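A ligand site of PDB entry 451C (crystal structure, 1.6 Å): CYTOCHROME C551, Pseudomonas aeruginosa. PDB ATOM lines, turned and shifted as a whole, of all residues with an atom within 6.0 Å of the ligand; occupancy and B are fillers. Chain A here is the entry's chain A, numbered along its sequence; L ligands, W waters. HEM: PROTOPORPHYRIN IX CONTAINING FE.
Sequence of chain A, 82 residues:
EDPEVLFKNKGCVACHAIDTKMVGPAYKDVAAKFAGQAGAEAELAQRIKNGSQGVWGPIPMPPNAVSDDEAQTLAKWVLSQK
N of Cys 12 sits close to O of Phe 7 (3.3 Å).
O of Cys 15 lies within hydrogen-bond range of N of Gly 24, at 2.9 Å.
O of Cys 15 lies within hydrogen-bond range of N of Val 23 (3.1 Å).
A ring nitrogen (ND1) of His 16 sits at hydrogen-bond distance from the backbone carbonyl oxygen (O) of Pro 25, 2.8 Å away.
The backbone carbonyl oxygen of Ser 52 lies within hydrogen-bond range of the backbone NH of Met 61, 2.7 Å away.
SD of Met 61 lies close to ND2 of Asn 64 (3.6 Å).
O of Pro 58 lies close to OE1 of Gln 53 (2.8 Å).
The side-chain amide nitrogen (ND2) of Asn 64 sits at hydrogen-bond distance from the backbone carbonyl oxygen (O) of Ile 48 (2.7 Å).
CAB of the ligand is bonded to SG of Cys 12.
The side-chain sulfur (SG) of Cys 15 is covalently linked to a carbon (CAC) of the ligand.
NE2 of His 16 binds FE of the ligand (2.0 Å).
The side-chain sulfur (SD) of Met 61 binds an iron atom (FE) of the ligand, 2.4 Å away.
The guanidinium group of Arg 47 is in salt-bridge range of an oxygen (O2A) of the ligand (2.6 Å).
The backbone NH (N) of Trp 56 sits at hydrogen-bond distance from an oxygen (O2D) of the ligand, at 2.8 Å.
The indole nitrogen (NE1) of Trp 56 sits at hydrogen-bond distance from an oxygen (O1A) of the ligand (2.8 Å).
The backbone NH (N) of Val 55 sits at hydrogen-bond distance from an oxygen (O1D) of the ligand (2.9 Å).
OG of Ser 52 lies within hydrogen-bond range of O1D of the ligand, at 3.0 Å.
O1D of the ligand sits at hydrogen-bond distance from N of Gly 54 (3.2 Å).
O1D of the ligand lies close to N of Gln 53, at 3.4 Å.
N of Gly 57 is in hydrogen-bond range of O2D of the ligand.
Residues that only touch the ligand: Phe 34 (3.3 Å), Tyr 27 (3.5 Å), Leu 44 (3.5 Å), Pro 25 (3.6 Å), Asn 64 (3.6 Å), Gly 24 (3.6 Å), Gly 11 (3.7 Å), Pro 60 (3.7 Å), Ile 48 (3.7 Å), Ile 59 (3.8 Å), Pro 62 (3.8 Å), Val 23 (3.9 Å) and Leu 74 (3.9 Å).
24 residues have an atom within 4 Å of the ligand: Gly 11, Cys 12, Cys 15, His 16, Val 23, Gly 24, Pro 25, Tyr 27, Phe 34, Leu 44, Arg 47, Ile 48, Ser 52, Gln 53, Gly 54, Val 55, Trp 56, Gly 57, Ile 59, Pro 60, Met 61, Pro 62, Asn 64 and Leu 74.
Along chain A the residues within 4 Å of the ligand span positions 11 to 74.
The nearest printed residue that does not touch the ligand is Lys 10 (4.03 Å).
Water W1 lies within hydrogen-bond range of an oxygen (O2D) of the ligand (2.6 Å), the backbone carbonyl oxygen of Ile 59 (2.6 Å) and the backbone carbonyl oxygen of Gly 57 (3.2 Å).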
ATOM      1  N   LEU A   6     -16.030  27.440   6.520  1.00  0.00           N
ATOM      2  CA  LEU A   6     -16.355  27.981   7.836  1.00  0.00           C
ATOM      3  C   LEU A   6     -15.325  27.565   8.883  1.00  0.00           C
ATOM      4  O   LEU A   6     -14.954  28.368   9.736  1.00  0.00           O
ATOM      5  CB  LEU A   6     -17.718  27.486   8.302  1.00  0.00           C
ATOM      6  CG  LEU A   6     -18.874  28.154   7.550  1.00  0.00           C
ATOM      7  CD1 LEU A   6     -20.190  27.439   7.820  1.00  0.00           C
ATOM      8  CD2 LEU A   6     -18.957  29.639   7.856  1.00  0.00           C
ATOM      9  N   PHE A   7     -14.936  26.319   8.828  1.00  0.00           N
ATOM     10  CA  PHE A   7     -13.982  25.775   9.809  1.00  0.00           C
ATOM     11  C   PHE A   7     -12.683  26.584   9.863  1.00  0.00           C
ATOM     12  O   PHE A   7     -12.175  26.896  10.946  1.00  0.00           O
ATOM     13  CB  PHE A   7     -13.673  24.334   9.409  1.00  0.00           C
ATOM     14  CG  PHE A   7     -12.492  23.689  10.114  1.00  0.00           C
ATOM     15  CD1 PHE A   7     -11.364  23.369   9.394  1.00  0.00           C
ATOM     16  CD2 PHE A   7     -12.563  23.393  11.458  1.00  0.00           C
ATOM     17  CE1 PHE A   7     -10.285  22.734  10.013  1.00  0.00           C
ATOM     18  CE2 PHE A   7     -11.492  22.758  12.100  1.00  0.00           C
ATOM     19  CZ  PHE A   7     -10.349  22.418  11.364  1.00  0.00           C
ATOM     20  N   LYS A  10     -13.938  30.830  10.599  1.00  0.00           N
ATOM     21  CA  LYS A  10     -14.456  31.205  11.923  1.00  0.00           C
ATOM     22  C   LYS A  10     -13.469  30.886  13.040  1.00  0.00           C
ATOM     23  O   LYS A  10     -13.775  31.087  14.225  1.00  0.00           O
ATOM     24  CB  LYS A  10     -15.761  30.477  12.188  1.00  0.00           C
ATOM     25  CG  LYS A  10     -16.823  30.856  11.179  1.00  0.00           C
ATOM     26  CD  LYS A  10     -17.300  32.278  11.386  1.00  0.00           C
ATOM     27  CE  LYS A  10     -18.362  32.656  10.360  1.00  0.00           C
ATOM     28  NZ  LYS A  10     -18.985  33.933  10.723  1.00  0.00           N
ATOM     29  N   GLY A  11     -12.261  30.524  12.656  1.00  0.00           N
ATOM     30  CA  GLY A  11     -11.195  30.338  13.660  1.00  0.00           C
ATOM     31  C   GLY A  11     -11.163  28.984  14.371  1.00  0.00           C
ATOM     32  O   GLY A  11     -10.374  28.795  15.304  1.00  0.00           O
ATOM     33  N   CYS A  12     -12.097  28.110  14.013  1.00  0.00           N
ATOM     34  CA  CYS A  12     -12.196  26.755  14.616  1.00  0.00           C
ATOM     35  C   CYS A  12     -10.863  26.019  14.542  1.00  0.00           C
ATOM     36  O   CYS A  12     -10.473  25.301  15.469  1.00  0.00           O
ATOM     37  CB  CYS A  12     -13.164  25.955  13.768  1.00  0.00           C
ATOM     38  SG  CYS A  12     -14.765  26.742  13.590  1.00  0.00           S
ATOM     39  N   VAL A  13     -10.212  26.236  13.412  1.00  0.00           N
ATOM     40  CA  VAL A  13      -8.928  25.601  13.067  1.00  0.00           C
ATOM     41  C   VAL A  13      -7.811  25.899  14.075  1.00  0.00           C
ATOM     42  O   VAL A  13      -6.847  25.128  14.190  1.00  0.00           O
ATOM     43  CB  VAL A  13      -8.532  25.990  11.648  1.00  0.00           C
ATOM     44  CG1 VAL A  13      -8.190  27.474  11.501  1.00  0.00           C
ATOM     45  CG2 VAL A  13      -7.470  25.096  11.028  1.00  0.00           C
ATOM     46  N   ALA A  14      -7.986  26.970  14.830  1.00  0.00           N
ATOM     47  CA  ALA A  14      -6.972  27.334  15.825  1.00  0.00           C
ATOM     48  C   ALA A  14      -7.005  26.436  17.053  1.00  0.00           C
ATOM     49  O   ALA A  14      -6.015  26.375  17.784  1.00  0.00           O
ATOM     50  CB  ALA A  14      -7.181  28.775  16.275  1.00  0.00           C
ATOM     51  N   CYS A  15      -8.138  25.808  17.309  1.00  0.00           N
ATOM     52  CA  CYS A  15      -8.272  24.998  18.529  1.00  0.00           C
ATOM     53  C   CYS A  15      -8.622  23.524  18.247  1.00  0.00           C
ATOM     54  O   CYS A  15      -8.715  22.716  19.171  1.00  0.00           O
ATOM     55  CB  CYS A  15      -9.398  25.562  19.396  1.00  0.00           C
ATOM     56  SG  CYS A  15      -9.003  27.167  20.119  1.00  0.00           S
ATOM     57  N   HIS A  16      -8.970  23.244  16.998  1.00  0.00           N
ATOM     58  CA  HIS A  16      -9.431  21.890  16.683  1.00  0.00           C
ATOM     59  C   HIS A  16      -8.751  21.319  15.437  1.00  0.00           C
ATOM     60  O   HIS A  16      -8.623  22.027  14.432  1.00  0.00           O
ATOM     61  CB  HIS A  16     -10.930  21.915  16.438  1.00  0.00           C
ATOM     62  CG  HIS A  16     -11.821  22.150  17.650  1.00  0.00           C
ATOM     63  ND1 HIS A  16     -12.135  21.161  18.525  1.00  0.00           N
ATOM     64  CD2 HIS A  16     -12.537  23.279  17.989  1.00  0.00           C
ATOM     65  CE1 HIS A  16     -13.031  21.670  19.408  1.00  0.00           C
ATOM     66  NE2 HIS A  16     -13.280  22.969  19.086  1.00  0.00           N
ATOM     67  N   VAL A  23      -6.460  22.217  21.310  1.00  0.00           N
ATOM     68  CA  VAL A  23      -7.009  22.845  22.521  1.00  0.00           C
ATOM     69  C   VAL A  23      -8.370  22.260  22.911  1.00  0.00           C
ATOM     70  O   VAL A  23      -8.565  21.852  24.062  1.00  0.00           O
ATOM     71  CB  VAL A  23      -7.181  24.346  22.307  1.00  0.00           C
ATOM     72  CG1 VAL A  23      -7.734  25.018  23.550  1.00  0.00           C
ATOM     73  CG2 VAL A  23      -5.887  24.988  21.816  1.00  0.00           C
ATOM     74  N   GLY A  24      -9.225  22.074  21.915  1.00  0.00           N
ATOM     75  CA  GLY A  24     -10.448  21.304  22.152  1.00  0.00           C
ATOM     76  C   GLY A  24     -10.308  19.897  21.580  1.00  0.00           C
ATOM     77  O   GLY A  24      -9.277  19.550  20.979  1.00  0.00           O
ATOM     78  N   PRO A  25     -11.313  19.081  21.752  1.00  0.00           N
ATOM     79  CA  PRO A  25     -11.332  17.680  21.269  1.00  0.00           C
ATOM     80  C   PRO A  25     -11.163  17.549  19.741  1.00  0.00           C
ATOM     81  O   PRO A  25     -11.580  18.424  18.979  1.00  0.00           O
ATOM     82  CB  PRO A  25     -12.695  17.146  21.680  1.00  0.00           C
ATOM     83  CG  PRO A  25     -13.551  18.378  21.894  1.00  0.00           C
ATOM     84  CD  PRO A  25     -12.587  19.436  22.414  1.00  0.00           C
ATOM     85  N   TYR A  27     -12.394  16.248  16.209  1.00  0.00           N
ATOM     86  CA  TYR A  27     -13.764  16.032  15.693  1.00  0.00           C
ATOM     87  C   TYR A  27     -14.166  14.564  15.510  1.00  0.00           C
ATOM     88  O   TYR A  27     -15.319  14.236  15.806  1.00  0.00           O
ATOM     89  CB  TYR A  27     -14.091  16.839  14.441  1.00  0.00           C
ATOM     90  CG  TYR A  27     -14.102  18.347  14.612  1.00  0.00           C
ATOM     91  CD1 TYR A  27     -13.696  19.166  13.572  1.00  0.00           C
ATOM     92  CD2 TYR A  27     -14.489  18.902  15.812  1.00  0.00           C
ATOM     93  CE1 TYR A  27     -13.667  20.551  13.749  1.00  0.00           C
ATOM     94  CE2 TYR A  27     -14.454  20.282  16.013  1.00  0.00           C
ATOM     95  CZ  TYR A  27     -14.025  21.104  14.972  1.00  0.00           C
ATOM     96  OH  TYR A  27     -13.968  22.407  15.159  1.00  0.00           O
ATOM     97  N   VAL A  30     -15.527  13.566  18.783  1.00  0.00           N
ATOM     98  CA  VAL A  30     -16.848  14.151  19.057  1.00  0.00           C
ATOM     99  C   VAL A  30     -17.928  13.379  18.314  1.00  0.00           C
ATOM    100  O   VAL A  30     -18.966  13.016  18.876  1.00  0.00           O
ATOM    101  CB  VAL A  30     -16.894  15.621  18.657  1.00  0.00           C
ATOM    102  CG1 VAL A  30     -18.275  16.207  18.851  1.00  0.00           C
ATOM    103  CG2 VAL A  30     -15.851  16.432  19.422  1.00  0.00           C
ATOM    104  N   LYS A  33     -18.562  10.040  19.989  1.00  0.00           N
ATOM    105  CA  LYS A  33     -19.407  10.109  21.193  1.00  0.00           C
ATOM    106  C   LYS A  33     -20.860  10.369  20.834  1.00  0.00           C
ATOM    107  O   LYS A  33     -21.773   9.758  21.403  1.00  0.00           O
ATOM    108  CB  LYS A  33     -18.928  11.170  22.202  1.00  0.00           C
ATOM    109  CG  LYS A  33     -19.894  11.316  23.386  1.00  0.00           C
ATOM    110  CD  LYS A  33     -19.226  11.557  24.741  1.00  0.00           C
ATOM    111  CE  LYS A  33     -18.587  12.929  24.861  1.00  0.00           C
ATOM    112  NZ  LYS A  33     -17.553  12.906  25.907  1.00  0.00           N
ATOM    113  N   PHE A  34     -21.077  11.281  19.910  1.00  0.00           N
ATOM    114  CA  PHE A  34     -22.478  11.649  19.701  1.00  0.00           C
ATOM    115  C   PHE A  34     -23.088  10.857  18.562  1.00  0.00           C
ATOM    116  O   PHE A  34     -24.291  10.985  18.340  1.00  0.00           O
ATOM    117  CB  PHE A  34     -22.616  13.142  19.516  1.00  0.00           C
ATOM    118  CG  PHE A  34     -22.252  13.860  20.785  1.00  0.00           C
ATOM    119  CD1 PHE A  34     -21.081  14.584  20.876  1.00  0.00           C
ATOM    120  CD2 PHE A  34     -23.061  13.722  21.896  1.00  0.00           C
ATOM    121  CE1 PHE A  34     -20.714  15.199  22.070  1.00  0.00           C
ATOM    122  CE2 PHE A  34     -22.719  14.334  23.108  1.00  0.00           C
ATOM    123  CZ  PHE A  34     -21.530  15.082  23.191  1.00  0.00           C
ATOM    124  N   GLU A  43     -28.014  20.054  19.494  1.00  0.00           N
ATOM    125  CA  GLU A  43     -27.331  20.292  20.768  1.00  0.00           C
ATOM    126  C   GLU A  43     -25.884  20.737  20.610  1.00  0.00           C
ATOM    127  O   GLU A  43     -25.477  21.750  21.184  1.00  0.00           O
ATOM    128  CB  GLU A  43     -27.582  19.146  21.744  1.00  0.00           C
ATOM    129  CG  GLU A  43     -29.091  19.081  21.944  1.00  0.00           C
ATOM    130  CD  GLU A  43     -29.527  18.171  23.100  1.00  0.00           C
ATOM    131  OE1 GLU A  43     -30.327  17.271  22.851  1.00  0.00           O
ATOM    132  OE2 GLU A  43     -29.366  18.608  24.251  1.00  0.00           O
ATOM    133  N   LEU A  44     -25.228  20.150  19.632  1.00  0.00           N
ATOM    134  CA  LEU A  44     -23.885  20.636  19.306  1.00  0.00           C
ATOM    135  C   LEU A  44     -23.938  22.053  18.724  1.00  0.00           C
ATOM    136  O   LEU A  44     -23.050  22.852  19.013  1.00  0.00           O
ATOM    137  CB  LEU A  44     -23.186  19.732  18.299  1.00  0.00           C
ATOM    138  CG  LEU A  44     -22.617  18.468  18.920  1.00  0.00           C
ATOM    139  CD1 LEU A  44     -21.822  17.681  17.887  1.00  0.00           C
ATOM    140  CD2 LEU A  44     -21.759  18.775  20.134  1.00  0.00           C
ATOM    141  N   ARG A  47     -23.974  24.556  21.381  1.00  0.00           N
ATOM    142  CA  ARG A  47     -22.700  24.658  22.091  1.00  0.00           C
ATOM    143  C   ARG A  47     -21.631  25.344  21.237  1.00  0.00           C
ATOM    144  O   ARG A  47     -20.827  26.132  21.765  1.00  0.00           O
ATOM    145  CB  ARG A  47     -22.244  23.289  22.598  1.00  0.00           C
ATOM    146  CG  ARG A  47     -23.258  22.681  23.568  1.00  0.00           C
ATOM    147  CD  ARG A  47     -22.772  21.404  24.260  1.00  0.00           C
ATOM    148  NE  ARG A  47     -23.911  20.489  24.510  1.00  0.00           N
ATOM    149  CZ  ARG A  47     -23.879  19.146  24.670  1.00  0.00           C
ATOM    150  NH1 ARG A  47     -25.024  18.524  24.810  1.00  0.00           N
ATOM    151  NH2 ARG A  47     -22.757  18.403  24.682  1.00  0.00           N
ATOM    152  N   ILE A  48     -21.659  25.095  19.951  1.00  0.00           N
ATOM    153  CA  ILE A  48     -20.727  25.819  19.069  1.00  0.00           C
ATOM    154  C   ILE A  48     -20.972  27.333  19.127  1.00  0.00           C
ATOM    155  O   ILE A  48     -20.032  28.111  19.300  1.00  0.00           O
ATOM    156  CB  ILE A  48     -20.872  25.325  17.632  1.00  0.00           C
ATOM    157  CG1 ILE A  48     -20.486  23.855  17.533  1.00  0.00           C
ATOM    158  CG2 ILE A  48     -20.091  26.165  16.612  1.00  0.00           C
ATOM    159  CD1 ILE A  48     -20.812  23.278  16.162  1.00  0.00           C
ATOM    160  N   SER A  52     -19.117  26.075  25.450  1.00  0.00           N
ATOM    161  CA  SER A  52     -19.217  24.773  26.125  1.00  0.00           C
ATOM    162  C   SER A  52     -18.177  24.654  27.235  1.00  0.00           C
ATOM    163  O   SER A  52     -17.057  25.143  27.080  1.00  0.00           O
ATOM    164  CB  SER A  52     -18.997  23.657  25.106  1.00  0.00           C
ATOM    165  OG  SER A  52     -19.243  22.391  25.725  1.00  0.00           O
ATOM    166  N   GLN A  53     -18.487  23.896  28.275  1.00  0.00           N
ATOM    167  CA  GLN A  53     -17.464  23.570  29.288  1.00  0.00           C
ATOM    168  C   GLN A  53     -17.802  22.268  29.997  1.00  0.00           C
ATOM    169  O   GLN A  53     -18.976  22.055  30.344  1.00  0.00           O
ATOM    170  CB  GLN A  53     -17.364  24.699  30.335  1.00  0.00           C
ATOM    171  CG  GLN A  53     -16.151  24.512  31.249  1.00  0.00           C
ATOM    172  CD  GLN A  53     -15.965  25.697  32.198  1.00  0.00           C
ATOM    173  OE1 GLN A  53     -14.874  25.873  32.740  1.00  0.00           O
ATOM    174  NE2 GLN A  53     -16.786  26.698  32.050  1.00  0.00           N
ATOM    175  N   GLY A  54     -16.800  21.463  30.310  1.00  0.00           N
ATOM    176  CA  GLY A  54     -17.072  20.339  31.209  1.00  0.00           C
ATOM    177  C   GLY A  54     -17.270  19.002  30.495  1.00  0.00           C
ATOM    178  O   GLY A  54     -17.167  17.944  31.117  1.00  0.00           O
ATOM    179  N   VAL A  55     -17.618  19.049  29.214  1.00  0.00           N
ATOM    180  CA  VAL A  55     -17.878  17.783  28.508  1.00  0.00           C
ATOM    181  C   VAL A  55     -16.601  17.004  28.172  1.00  0.00           C
ATOM    182  O   VAL A  55     -16.585  15.768  28.240  1.00  0.00           O
ATOM    183  CB  VAL A  55     -18.739  18.017  27.267  1.00  0.00           C
ATOM    184  CG1 VAL A  55     -19.146  16.712  26.577  1.00  0.00           C
ATOM    185  CG2 VAL A  55     -19.952  18.875  27.597  1.00  0.00           C
ATOM    186  N   TRP A  56     -15.558  17.743  27.807  1.00  0.00           N
ATOM    187  CA  TRP A  56     -14.313  17.103  27.359  1.00  0.00           C
ATOM    188  C   TRP A  56     -13.117  17.462  28.229  1.00  0.00           C
ATOM    189  O   TRP A  56     -11.965  17.186  27.865  1.00  0.00           O
ATOM    190  CB  TRP A  56     -13.988  17.527  25.933  1.00  0.00           C
ATOM    191  CG  TRP A  56     -15.035  17.067  24.951  1.00  0.00           C
ATOM    192  CD1 TRP A  56     -16.171  17.734  24.528  1.00  0.00           C
ATOM    193  CD2 TRP A  56     -15.086  15.824  24.309  1.00  0.00           C
ATOM    194  NE1 TRP A  56     -16.870  16.919  23.670  1.00  0.00           N
ATOM    195  CE2 TRP A  56     -16.253  15.811  23.534  1.00  0.00           C
ATOM    196  CE3 TRP A  56     -14.228  14.729  24.364  1.00  0.00           C
ATOM    197  CZ2 TRP A  56     -16.620  14.727  22.755  1.00  0.00           C
ATOM    198  CZ3 TRP A  56     -14.597  13.624  23.581  1.00  0.00           C
ATOM    199  CH2 TRP A  56     -15.757  13.625  22.799  1.00  0.00           C
ATOM    200  N   GLY A  57     -13.416  18.170  29.297  1.00  0.00           N
ATOM    201  CA  GLY A  57     -12.346  18.684  30.166  1.00  0.00           C
ATOM    202  C   GLY A  57     -12.807  19.985  30.831  1.00  0.00           C
ATOM    203  O   GLY A  57     -13.970  20.336  30.688  1.00  0.00           O
ATOM    204  N   PRO A  58     -11.934  20.577  31.647  1.00  0.00           N
ATOM    205  CA  PRO A  58     -12.300  21.689  32.536  1.00  0.00           C
ATOM    206  C   PRO A  58     -12.266  23.052  31.847  1.00  0.00           C
ATOM    207  O   PRO A  58     -12.723  24.035  32.433  1.00  0.00           O
ATOM    208  CB  PRO A  58     -11.254  21.656  33.646  1.00  0.00           C
ATOM    209  CG  PRO A  58     -10.027  21.080  32.981  1.00  0.00           C
ATOM    210  CD  PRO A  58     -10.580  20.061  31.994  1.00  0.00           C
ATOM    211  N   ILE A  59     -11.663  23.118  30.669  1.00  0.00           N
ATOM    212  CA  ILE A  59     -11.513  24.412  29.992  1.00  0.00           C
ATOM    213  C   ILE A  59     -12.626  24.669  28.968  1.00  0.00           C
ATOM    214  O   ILE A  59     -13.163  23.732  28.381  1.00  0.00           O
ATOM    215  CB  ILE A  59     -10.133  24.564  29.361  1.00  0.00           C
ATOM    216  CG1 ILE A  59      -9.938  23.696  28.119  1.00  0.00           C
ATOM    217  CG2 ILE A  59      -9.023  24.391  30.375  1.00  0.00           C
ATOM    218  CD1 ILE A  59      -8.675  24.099  27.377  1.00  0.00           C
ATOM    219  N   PRO A  60     -13.055  25.908  28.868  1.00  0.00           N
ATOM    220  CA  PRO A  60     -14.231  26.257  28.071  1.00  0.00           C
ATOM    221  C   PRO A  60     -13.888  26.429  26.590  1.00  0.00           C
ATOM    222  O   PRO A  60     -12.849  26.997  26.236  1.00  0.00           O
ATOM    223  CB  PRO A  60     -14.683  27.596  28.636  1.00  0.00           C
ATOM    224  CG  PRO A  60     -13.402  28.241  29.099  1.00  0.00           C
ATOM    225  CD  PRO A  60     -12.549  27.086  29.609  1.00  0.00           C
ATOM    226  N   MET A  61     -14.889  26.171  25.792  1.00  0.00           N
ATOM    227  CA  MET A  61     -14.913  26.770  24.455  1.00  0.00           C
ATOM    228  C   MET A  61     -15.685  28.072  24.588  1.00  0.00           C
ATOM    229  O   MET A  61     -16.855  28.034  25.012  1.00  0.00           O
ATOM    230  CB  MET A  61     -15.700  25.907  23.474  1.00  0.00           C
ATOM    231  CG  MET A  61     -15.786  26.611  22.115  1.00  0.00           C
ATOM    232  SD  MET A  61     -16.329  25.556  20.736  1.00  0.00           S
ATOM    233  CE  MET A  61     -17.777  24.659  21.344  1.00  0.00           C
ATOM    234  N   PRO A  62     -15.020  29.191  24.347  1.00  0.00           N
ATOM    235  CA  PRO A  62     -15.645  30.532  24.330  1.00  0.00           C
ATOM    236  C   PRO A  62     -16.712  30.606  23.247  1.00  0.00           C
ATOM    237  O   PRO A  62     -16.600  29.891  22.229  1.00  0.00           O
ATOM    238  CB  PRO A  62     -14.519  31.489  23.968  1.00  0.00           C
ATOM    239  CG  PRO A  62     -13.231  30.705  24.147  1.00  0.00           C
ATOM    240  CD  PRO A  62     -13.627  29.269  23.876  1.00  0.00           C
ATOM    241  N   ASN A  64     -18.707  31.560  20.000  1.00  0.00           N
ATOM    242  CA  ASN A  64     -18.161  31.817  18.667  1.00  0.00           C
ATOM    243  C   ASN A  64     -18.949  32.904  17.951  1.00  0.00           C
ATOM    244  O   ASN A  64     -20.118  33.139  18.272  1.00  0.00           O
ATOM    245  CB  ASN A  64     -18.178  30.525  17.848  1.00  0.00           C
ATOM    246  CG  ASN A  64     -17.017  29.627  18.296  1.00  0.00           C
ATOM    247  OD1 ASN A  64     -15.849  29.955  18.086  1.00  0.00           O
ATOM    248  ND2 ASN A  64     -17.343  28.516  18.941  1.00  0.00           N
ATOM    249  N   VAL A  66     -20.502  33.019  15.168  1.00  0.00           N
ATOM    250  CA  VAL A  66     -21.218  32.325  14.101  1.00  0.00           C
ATOM    251  C   VAL A  66     -22.718  32.571  14.231  1.00  0.00           C
ATOM    252  O   VAL A  66     -23.213  32.779  15.333  1.00  0.00           O
ATOM    253  CB  VAL A  66     -20.961  30.803  14.141  1.00  0.00           C
ATOM    254  CG1 VAL A  66     -19.574  30.409  13.676  1.00  0.00           C
ATOM    255  CG2 VAL A  66     -21.333  30.176  15.482  1.00  0.00           C
ATOM    256  N   LEU A  74     -21.966  23.592  10.739  1.00  0.00           N
ATOM    257  CA  LEU A  74     -20.750  23.081  11.354  1.00  0.00           C
ATOM    258  C   LEU A  74     -21.025  21.839  12.203  1.00  0.00           C
ATOM    259  O   LEU A  74     -20.245  20.885  12.153  1.00  0.00           O
ATOM    260  CB  LEU A  74     -20.103  24.176  12.207  1.00  0.00           C
ATOM    261  CG  LEU A  74     -19.304  25.186  11.380  1.00  0.00           C
ATOM    262  CD1 LEU A  74     -19.016  26.465  12.142  1.00  0.00           C
ATOM    263  CD2 LEU A  74     -18.021  24.580  10.819  1.00  0.00           C
ATOM    264  N   ALA A  75     -22.108  21.867  12.968  1.00  0.00           N
ATOM    265  CA  ALA A  75     -22.429  20.697  13.813  1.00  0.00           C
ATOM    266  C   ALA A  75     -22.640  19.438  12.973  1.00  0.00           C
ATOM    267  O   ALA A  75     -22.108  18.374  13.298  1.00  0.00           O
ATOM    268  CB  ALA A  75     -23.701  20.968  14.602  1.00  0.00           C
ATOM    269  N   VAL A  78     -19.258  18.249  11.690  1.00  0.00           N
ATOM    270  CA  VAL A  78     -18.494  17.565  12.769  1.00  0.00           C
ATOM    271  C   VAL A  78     -19.001  16.145  13.020  1.00  0.00           C
ATOM    272  O   VAL A  78     -18.214  15.190  13.062  1.00  0.00           O
ATOM    273  CB  VAL A  78     -18.555  18.367  14.064  1.00  0.00           C
ATOM    274  CG1 VAL A  78     -18.039  17.588  15.270  1.00  0.00           C
ATOM    275  CG2 VAL A  78     -17.832  19.700  13.925  1.00  0.00           C
HETATM  276  CHA HEM L   1     -15.642  21.689  22.112  1.00  0.00           C
HETATM  277  CHB HEM L   1     -16.862  22.933  17.623  1.00  0.00           C
HETATM  278  CHC HEM L   1     -13.942  26.773  17.905  1.00  0.00           C
HETATM  279  CHD HEM L   1     -12.266  25.150  22.124  1.00  0.00           C
HETATM  280  C1A HEM L   1     -16.253  21.712  20.878  1.00  0.00           C
HETATM  281  C2A HEM L   1     -17.201  20.804  20.447  1.00  0.00           C
HETATM  282  C3A HEM L   1     -17.507  21.132  19.138  1.00  0.00           C
HETATM  283  C4A HEM L   1     -16.792  22.262  18.831  1.00  0.00           C
HETATM  284  CMA HEM L   1     -18.481  20.428  18.209  1.00  0.00           C
HETATM  285  CAA HEM L   1     -17.794  19.698  21.271  1.00  0.00           C
HETATM  286  CBA HEM L   1     -18.913  20.297  22.101  1.00  0.00           C
HETATM  287  CGA HEM L   1     -19.551  19.231  22.969  1.00  0.00           C
HETATM  288  O1A HEM L   1     -19.273  18.048  22.774  1.00  0.00           O
HETATM  289  O2A HEM L   1     -20.728  19.522  23.420  1.00  0.00           O
HETATM  290  C1B HEM L   1     -16.165  24.073  17.293  1.00  0.00           C
HETATM  291  C2B HEM L   1     -16.313  24.778  16.103  1.00  0.00           C
HETATM  292  C3B HEM L   1     -15.542  25.938  16.210  1.00  0.00           C
HETATM  293  C4B HEM L   1     -14.865  25.852  17.440  1.00  0.00           C
HETATM  294  CMB HEM L   1     -17.209  24.384  14.946  1.00  0.00           C
HETATM  295  CAB HEM L   1     -15.453  27.100  15.236  1.00  0.00           C
HETATM  296  CBB HEM L   1     -16.749  27.901  15.132  1.00  0.00           C
HETATM  297  C1C HEM L   1     -13.240  26.673  19.101  1.00  0.00           C
HETATM  298  C2C HEM L   1     -12.226  27.538  19.499  1.00  0.00           C
HETATM  299  C3C HEM L   1     -11.636  26.971  20.626  1.00  0.00           C
HETATM  300  C4C HEM L   1     -12.432  25.905  20.983  1.00  0.00           C
HETATM  301  CMC HEM L   1     -11.752  28.761  18.745  1.00  0.00           C
HETATM  302  CAC HEM L   1     -10.355  27.380  21.330  1.00  0.00           C
HETATM  303  CBC HEM L   1     -10.412  28.784  21.912  1.00  0.00           C
HETATM  304  C1D HEM L   1     -13.064  24.099  22.497  1.00  0.00           C
HETATM  305  C2D HEM L   1     -12.951  23.419  23.710  1.00  0.00           C
HETATM  306  C3D HEM L   1     -13.973  22.486  23.745  1.00  0.00           C
HETATM  307  C4D HEM L   1     -14.631  22.547  22.521  1.00  0.00           C
HETATM  308  CMD HEM L   1     -11.931  23.690  24.802  1.00  0.00           C
HETATM  309  CAD HEM L   1     -14.317  21.558  24.888  1.00  0.00           C
HETATM  310  CBD HEM L   1     -15.497  22.049  25.709  1.00  0.00           C
HETATM  311  CGD HEM L   1     -15.859  21.022  26.766  1.00  0.00           C
HETATM  312  O1D HEM L   1     -17.032  20.975  27.167  1.00  0.00           O
HETATM  313  O2D HEM L   1     -14.926  20.425  27.496  1.00  0.00           O
HETATM  314  NA  HEM L   1     -16.015  22.592  19.890  1.00  0.00           N
HETATM  315  NB  HEM L   1     -15.267  24.724  18.082  1.00  0.00           N
HETATM  316  NC  HEM L   1     -13.360  25.690  20.018  1.00  0.00           N
HETATM  317  ND  HEM L   1     -14.098  23.563  21.774  1.00  0.00           N
HETATM  318 FE   HEM L   1     -14.636  24.118  19.946  1.00  0.00          FE
HETATM  319  O   HOH W   1     -12.482  21.224  27.957  1.00  0.00           O
